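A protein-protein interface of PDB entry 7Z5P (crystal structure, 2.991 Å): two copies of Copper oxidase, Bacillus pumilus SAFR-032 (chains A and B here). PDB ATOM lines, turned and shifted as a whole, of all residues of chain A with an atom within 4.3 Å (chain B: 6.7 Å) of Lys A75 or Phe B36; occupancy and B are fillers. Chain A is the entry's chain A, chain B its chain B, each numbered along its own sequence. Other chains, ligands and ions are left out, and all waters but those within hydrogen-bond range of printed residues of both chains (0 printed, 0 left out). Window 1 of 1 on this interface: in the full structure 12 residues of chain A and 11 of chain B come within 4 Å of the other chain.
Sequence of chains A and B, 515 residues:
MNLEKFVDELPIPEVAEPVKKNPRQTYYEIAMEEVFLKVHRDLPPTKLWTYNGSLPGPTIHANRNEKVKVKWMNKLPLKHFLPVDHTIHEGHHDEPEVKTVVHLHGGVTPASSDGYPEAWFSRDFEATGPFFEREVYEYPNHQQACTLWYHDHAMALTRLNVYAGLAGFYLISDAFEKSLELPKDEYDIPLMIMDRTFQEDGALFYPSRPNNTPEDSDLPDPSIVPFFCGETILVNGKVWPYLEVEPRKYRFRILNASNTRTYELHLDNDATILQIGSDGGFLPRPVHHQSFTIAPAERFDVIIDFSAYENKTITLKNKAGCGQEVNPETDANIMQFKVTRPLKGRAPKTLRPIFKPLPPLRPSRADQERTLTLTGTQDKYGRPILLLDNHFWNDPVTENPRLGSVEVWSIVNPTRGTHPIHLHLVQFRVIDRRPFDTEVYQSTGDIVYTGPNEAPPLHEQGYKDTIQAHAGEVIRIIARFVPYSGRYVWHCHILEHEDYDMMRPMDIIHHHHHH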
ATOM      1  N   ALA A  31     -16.337  21.173 -27.180  1.00  0.00           N
ATOM      2  CA  ALA A  31     -17.051  20.408 -26.175  1.00  0.00           C
ATOM      3  C   ALA A  31     -18.457  20.959 -26.015  1.00  0.00           C
ATOM      4  O   ALA A  31     -18.666  22.172 -26.035  1.00  0.00           O
ATOM      5  CB  ALA A  31     -16.309  20.464 -24.851  1.00  0.00           C
ATOM      6  N   MET A  32     -19.420  20.047 -25.859  1.00  0.00           N
ATOM      7  CA  MET A  32     -20.801  20.386 -25.579  1.00  0.00           C
ATOM      8  C   MET A  32     -20.951  20.411 -24.063  1.00  0.00           C
ATOM      9  O   MET A  32     -20.598  19.438 -23.393  1.00  0.00           O
ATOM     10  CB  MET A  32     -21.731  19.338 -26.188  1.00  0.00           C
ATOM     11  CG  MET A  32     -21.526  19.076 -27.669  1.00  0.00           C
ATOM     12  SD  MET A  32     -22.193  17.460 -28.103  1.00  0.00           S
ATOM     13  CE  MET A  32     -21.179  17.016 -29.506  1.00  0.00           C
ATOM     14  N   GLU A  33     -21.464  21.531 -23.537  1.00  0.00           N
ATOM     15  CA  GLU A  33     -21.607  21.767 -22.095  1.00  0.00           C
ATOM     16  C   GLU A  33     -22.947  22.404 -21.761  1.00  0.00           C
ATOM     17  O   GLU A  33     -23.539  23.093 -22.595  1.00  0.00           O
ATOM     18  CB  GLU A  33     -20.468  22.652 -21.541  1.00  0.00           C
ATOM     19  CG  GLU A  33     -19.913  23.718 -22.483  1.00  0.00           C
ATOM     20  CD  GLU A  33     -18.649  24.372 -21.953  1.00  0.00           C
ATOM     21  OE1 GLU A  33     -17.762  23.664 -21.427  1.00  0.00           O
ATOM     22  OE2 GLU A  33     -18.530  25.606 -22.072  1.00  0.00           O
ATOM     23  N   MET A  73     -16.910  16.803 -28.555  1.00  0.00           N
ATOM     24  CA  MET A  73     -16.960  16.091 -27.280  1.00  0.00           C
ATOM     25  C   MET A  73     -18.296  16.300 -26.575  1.00  0.00           C
ATOM     26  O   MET A  73     -18.898  17.368 -26.670  1.00  0.00           O
ATOM     27  CB  MET A  73     -15.821  16.554 -26.373  1.00  0.00           C
ATOM     28  CG  MET A  73     -14.452  16.082 -26.829  1.00  0.00           C
ATOM     29  SD  MET A  73     -13.097  16.936 -25.999  1.00  0.00           S
ATOM     30  CE  MET A  73     -13.125  18.519 -26.839  1.00  0.00           C
ATOM     31  N   ASN A  74     -18.746  15.261 -25.863  1.00  0.00           N
ATOM     32  CA  ASN A  74     -19.963  15.297 -25.063  1.00  0.00           C
ATOM     33  C   ASN A  74     -19.597  15.467 -23.597  1.00  0.00           C
ATOM     34  O   ASN A  74     -19.067  14.543 -22.973  1.00  0.00           O
ATOM     35  CB  ASN A  74     -20.760  14.005 -25.256  1.00  0.00           C
ATOM     36  CG  ASN A  74     -22.071  13.994 -24.482  1.00  0.00           C
ATOM     37  OD1 ASN A  74     -22.305  14.823 -23.593  1.00  0.00           O
ATOM     38  ND2 ASN A  74     -22.935  13.036 -24.816  1.00  0.00           N
ATOM     39  N   LYS A  75     -19.866  16.661 -23.057  1.00  0.00           N
ATOM     40  CA  LYS A  75     -19.675  16.945 -21.640  1.00  0.00           C
ATOM     41  C   LYS A  75     -21.012  17.419 -21.060  1.00  0.00           C
ATOM     42  O   LYS A  75     -21.070  18.425 -20.352  1.00  0.00           O
ATOM     43  CB  LYS A  75     -18.567  17.988 -21.427  1.00  0.00           C
ATOM     44  CG  LYS A  75     -17.315  17.797 -22.286  1.00  0.00           C
ATOM     45  CD  LYS A  75     -16.522  16.542 -21.958  1.00  0.00           C
ATOM     46  CE  LYS A  75     -15.463  16.788 -20.903  1.00  0.00           C
ATOM     47  NZ  LYS A  75     -14.485  15.674 -20.765  1.00  0.00           N
ATOM     48  N   LEU A  76     -22.079  16.672 -21.372  1.00  0.00           N
ATOM     49  CA  LEU A  76     -23.436  16.981 -20.928  1.00  0.00           C
ATOM     50  C   LEU A  76     -23.815  16.156 -19.702  1.00  0.00           C
ATOM     51  O   LEU A  76     -23.165  15.155 -19.404  1.00  0.00           O
ATOM     52  CB  LEU A  76     -24.442  16.691 -22.047  1.00  0.00           C
ATOM     53  CG  LEU A  76     -24.644  17.777 -23.104  1.00  0.00           C
ATOM     54  CD1 LEU A  76     -25.461  18.925 -22.553  1.00  0.00           C
ATOM     55  CD2 LEU A  76     -23.328  18.318 -23.599  1.00  0.00           C
ATOM     56  N   ARG A 123     -21.718  11.032 -22.829  1.00  0.00           N
ATOM     57  CA  ARG A 123     -20.614  11.781 -22.163  1.00  0.00           C
ATOM     58  C   ARG A 123     -19.281  11.052 -22.383  1.00  0.00           C
ATOM     59  O   ARG A 123     -19.227   9.826 -22.149  1.00  0.00           O
ATOM     60  CB  ARG A 123     -20.917  11.953 -20.670  1.00  0.00           C
ATOM     61  CG  ARG A 123     -19.998  12.926 -19.943  1.00  0.00           C
ATOM     62  CD  ARG A 123     -20.295  12.938 -18.455  1.00  0.00           C
ATOM     63  NE  ARG A 123     -19.389  13.816 -17.723  1.00  0.00           N
ATOM     64  CZ  ARG A 123     -19.674  15.046 -17.294  1.00  0.00           C
ATOM     65  NH1 ARG A 123     -20.866  15.579 -17.507  1.00  0.00           N
ATOM     66  NH2 ARG A 123     -18.758  15.740 -16.641  1.00  0.00           N
ATOM     67  N   ASP A 124     -18.259  11.789 -22.842  1.00  0.00           N
ATOM     68  CA  ASP A 124     -16.907  11.275 -23.100  1.00  0.00           C
ATOM     69  C   ASP A 124     -16.880   9.895 -23.768  1.00  0.00           C
ATOM     70  O   ASP A 124     -16.027   9.061 -23.453  1.00  0.00           O
ATOM     71  CB  ASP A 124     -16.089  11.265 -21.798  1.00  0.00           C
ATOM     72  CG  ASP A 124     -15.705  12.661 -21.335  1.00  0.00           C
ATOM     73  OD1 ASP A 124     -15.435  13.520 -22.198  1.00  0.00           O
ATOM     74  OD2 ASP A 124     -15.652  12.877 -20.104  1.00  0.00           O
ATOM     75  N   GLU B  34     -19.880  24.918 -13.632  1.00  0.00           N
ATOM     76  CA  GLU B  34     -18.856  23.948 -14.010  1.00  0.00           C
ATOM     77  C   GLU B  34     -18.783  23.922 -15.528  1.00  0.00           C
ATOM     78  O   GLU B  34     -19.802  23.743 -16.195  1.00  0.00           O
ATOM     79  CB  GLU B  34     -19.186  22.548 -13.484  1.00  0.00           C
ATOM     80  CG  GLU B  34     -18.119  21.504 -13.781  1.00  0.00           C
ATOM     81  CD  GLU B  34     -18.449  20.143 -13.197  1.00  0.00           C
ATOM     82  OE1 GLU B  34     -19.458  19.544 -13.620  1.00  0.00           O
ATOM     83  OE2 GLU B  34     -17.689  19.667 -12.324  1.00  0.00           O
ATOM     84  N   VAL B  35     -17.574  24.113 -16.066  1.00  0.00           N
ATOM     85  CA  VAL B  35     -17.332  24.086 -17.508  1.00  0.00           C
ATOM     86  C   VAL B  35     -16.007  23.400 -17.811  1.00  0.00           C
ATOM     87  O   VAL B  35     -15.209  23.148 -16.911  1.00  0.00           O
ATOM     88  CB  VAL B  35     -17.340  25.502 -18.125  1.00  0.00           C
ATOM     89  CG1 VAL B  35     -18.719  26.135 -17.985  1.00  0.00           C
ATOM     90  CG2 VAL B  35     -16.273  26.386 -17.491  1.00  0.00           C
ATOM     91  N   PHE B  36     -15.796  23.087 -19.093  1.00  0.00           N
ATOM     92  CA  PHE B  36     -14.589  22.413 -19.559  1.00  0.00           C
ATOM     93  C   PHE B  36     -13.815  23.362 -20.456  1.00  0.00           C
ATOM     94  O   PHE B  36     -14.298  23.740 -21.521  1.00  0.00           O
ATOM     95  CB  PHE B  36     -14.952  21.134 -20.304  1.00  0.00           C
ATOM     96  CG  PHE B  36     -15.433  20.038 -19.401  1.00  0.00           C
ATOM     97  CD1 PHE B  36     -14.529  19.173 -18.808  1.00  0.00           C
ATOM     98  CD2 PHE B  36     -16.786  19.902 -19.103  1.00  0.00           C
ATOM     99  CE1 PHE B  36     -14.966  18.163 -17.965  1.00  0.00           C
ATOM    100  CE2 PHE B  36     -17.225  18.904 -18.255  1.00  0.00           C
ATOM    101  CZ  PHE B  36     -16.315  18.030 -17.689  1.00  0.00           C
ATOM    102  N   LEU B  37     -12.619  23.761 -20.005  1.00  0.00           N
ATOM    103  CA  LEU B  37     -11.824  24.769 -20.695  1.00  0.00           C
ATOM    104  C   LEU B  37     -10.449  24.250 -21.076  1.00  0.00           C
ATOM    105  O   LEU B  37      -9.864  23.426 -20.364  1.00  0.00           O
ATOM    106  CB  LEU B  37     -11.682  26.028 -19.836  1.00  0.00           C
ATOM    107  CG  LEU B  37     -12.984  26.703 -19.390  1.00  0.00           C
ATOM    108  CD1 LEU B  37     -12.684  28.016 -18.681  1.00  0.00           C
ATOM    109  CD2 LEU B  37     -13.932  26.939 -20.559  1.00  0.00           C
ATOM    110  N   LYS B  38      -9.955  24.740 -22.219  1.00  0.00           N
ATOM    111  CA  LYS B  38      -8.634  24.433 -22.721  1.00  0.00           C
ATOM    112  C   LYS B  38      -7.616  25.200 -21.876  1.00  0.00           C
ATOM    113  O   LYS B  38      -7.576  26.424 -21.900  1.00  0.00           O
ATOM    114  CB  LYS B  38      -8.551  24.749 -24.225  1.00  0.00           C
ATOM    115  CG  LYS B  38      -7.220  24.432 -24.899  1.00  0.00           C
ATOM    116  CD  LYS B  38      -6.838  22.962 -24.789  1.00  0.00           C
ATOM    117  CE  LYS B  38      -7.089  22.198 -26.073  1.00  0.00           C
ATOM    118  NZ  LYS B  38      -6.440  20.856 -26.043  1.00  0.00           N
ATOM    119  N   PRO B  45      -9.671  18.432 -22.314  1.00  0.00           N
ATOM    120  CA  PRO B  45     -10.492  19.389 -21.557  1.00  0.00           C
ATOM    121  C   PRO B  45     -10.212  19.326 -20.047  1.00  0.00           C
ATOM    122  O   PRO B  45     -10.023  18.239 -19.530  1.00  0.00           O
ATOM    123  CB  PRO B  45     -11.931  18.929 -21.835  1.00  0.00           C
ATOM    124  CG  PRO B  45     -11.838  18.203 -23.158  1.00  0.00           C
ATOM    125  CD  PRO B  45     -10.484  17.525 -23.126  1.00  0.00           C
ATOM    126  N   THR B  46     -10.210  20.488 -19.385  1.00  0.00           N
ATOM    127  CA  THR B  46      -9.938  20.557 -17.924  1.00  0.00           C
ATOM    128  C   THR B  46     -11.191  21.033 -17.176  1.00  0.00           C
ATOM    129  O   THR B  46     -11.447  22.253 -17.173  1.00  0.00           O
ATOM    130  CB  THR B  46      -8.733  21.461 -17.629  1.00  0.00           C
ATOM    131  OG1 THR B  46      -7.664  21.065 -18.488  1.00  0.00           O
ATOM    132  CG2 THR B  46      -8.284  21.390 -16.185  1.00  0.00           C
ATOM    133  N   LYS B  47     -11.931  20.097 -16.574  1.00  0.00           N
ATOM    134  CA  LYS B  47     -13.126  20.415 -15.812  1.00  0.00           C
ATOM    135  C   LYS B  47     -12.756  21.422 -14.743  1.00  0.00           C
ATOM    136  O   LYS B  47     -11.877  21.162 -13.924  1.00  0.00           O
ATOM    137  CB  LYS B  47     -13.692  19.161 -15.142  1.00  0.00           C
ATOM    138  CG  LYS B  47     -15.068  19.363 -14.527  1.00  0.00           C
ATOM    139  CD  LYS B  47     -15.761  18.036 -14.273  1.00  0.00           C
ATOM    140  CE  LYS B  47     -15.210  17.338 -13.049  1.00  0.00           C
ATOM    141  NZ  LYS B  47     -15.907  16.047 -12.800  1.00  0.00           N
ATOM    142  N   LEU B  48     -13.439  22.570 -14.761  1.00  0.00           N
ATOM    143  CA  LEU B  48     -13.199  23.662 -13.832  1.00  0.00           C
ATOM    144  C   LEU B  48     -14.521  24.224 -13.339  1.00  0.00           C
ATOM    145  O   LEU B  48     -15.542  24.132 -14.027  1.00  0.00           O
ATOM    146  CB  LEU B  48     -12.406  24.782 -14.513  1.00  0.00           C
ATOM    147  CG  LEU B  48     -11.079  24.410 -15.179  1.00  0.00           C
ATOM    148  CD1 LEU B  48     -10.578  25.567 -16.028  1.00  0.00           C
ATOM    149  CD2 LEU B  48     -10.039  24.016 -14.141  1.00  0.00           C
ATOM    150  N   ASP B 201      -5.055  12.798 -18.518  1.00  0.00           N
ATOM    151  CA  ASP B 201      -6.413  12.945 -19.047  1.00  0.00           C
ATOM    152  C   ASP B 201      -6.917  14.394 -19.079  1.00  0.00           C
ATOM    153  O   ASP B 201      -8.081  14.637 -19.396  1.00  0.00           O
ATOM    154  CB  ASP B 201      -7.391  12.086 -18.233  1.00  0.00           C
ATOM    155  CG  ASP B 201      -7.630  12.629 -16.828  1.00  0.00           C
ATOM    156  OD1 ASP B 201      -6.897  13.543 -16.395  1.00  0.00           O
ATOM    157  OD2 ASP B 201      -8.556  12.135 -16.154  1.00  0.00           O
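The side-chain carboxylate of Glu A33 lies within hydrogen-bond range of the backbone NH of Phe B36 (3.1 Å).
O of Leu A76 sits at hydrogen-bond distance from NH1 of Arg A123.
The backbone carbonyl oxygen (O) of Met A32 lies within hydrogen-bond range of the backbone NH (N) of Lys A75 (2.9 Å).
N of Met A32 sits at hydrogen-bond distance from O of Met A73 (2.8 Å).
ND2 of Asn A74 lies close to N of Arg A123, at 3.1 Å.
O of Val B35 is in hydrogen-bond range of N of Leu B48 (2.8 Å).
NZ of Lys A75 is in salt-bridge range of OD1 of Asp A124 (2.8 Å).
Among the printed residues, merely in contact across the chains: Lys A75 with Phe B36, Met A73 with Pro B45, Arg A123 with Phe B36 and Glu A33 with Val B35.
Of the printed residues of chain B, Glu A33 touches Val B35 and Phe B36.
Of the printed residues of chain B, Met A73 touches Pro B45 (3.4 Å).
Printed residues of chain B within 4 Å of Lys A75: Phe B36 (3.3 Å).
Printed residues of chain B within 4 Å of Arg A123: Phe B36.
Of the printed residues of chain A, Val B35 touches Glu A33 (3.8 Å).
Phe B36 touches three residues of chain A.
Printed residues of chain A within 4 Å of Pro B45: Met A73.
Thr B46 touches none of the printed residues of chain A.
Asp B201 touches none of the printed residues of chain A.
Along chain B the printed residues that touch a printed residue of chain A span positions 35 to 45.
Printed residues of chain A that touch a printed residue of chain B: Glu A33, Met A73, Lys A75 and Arg A123.
No position is printed for both chains.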
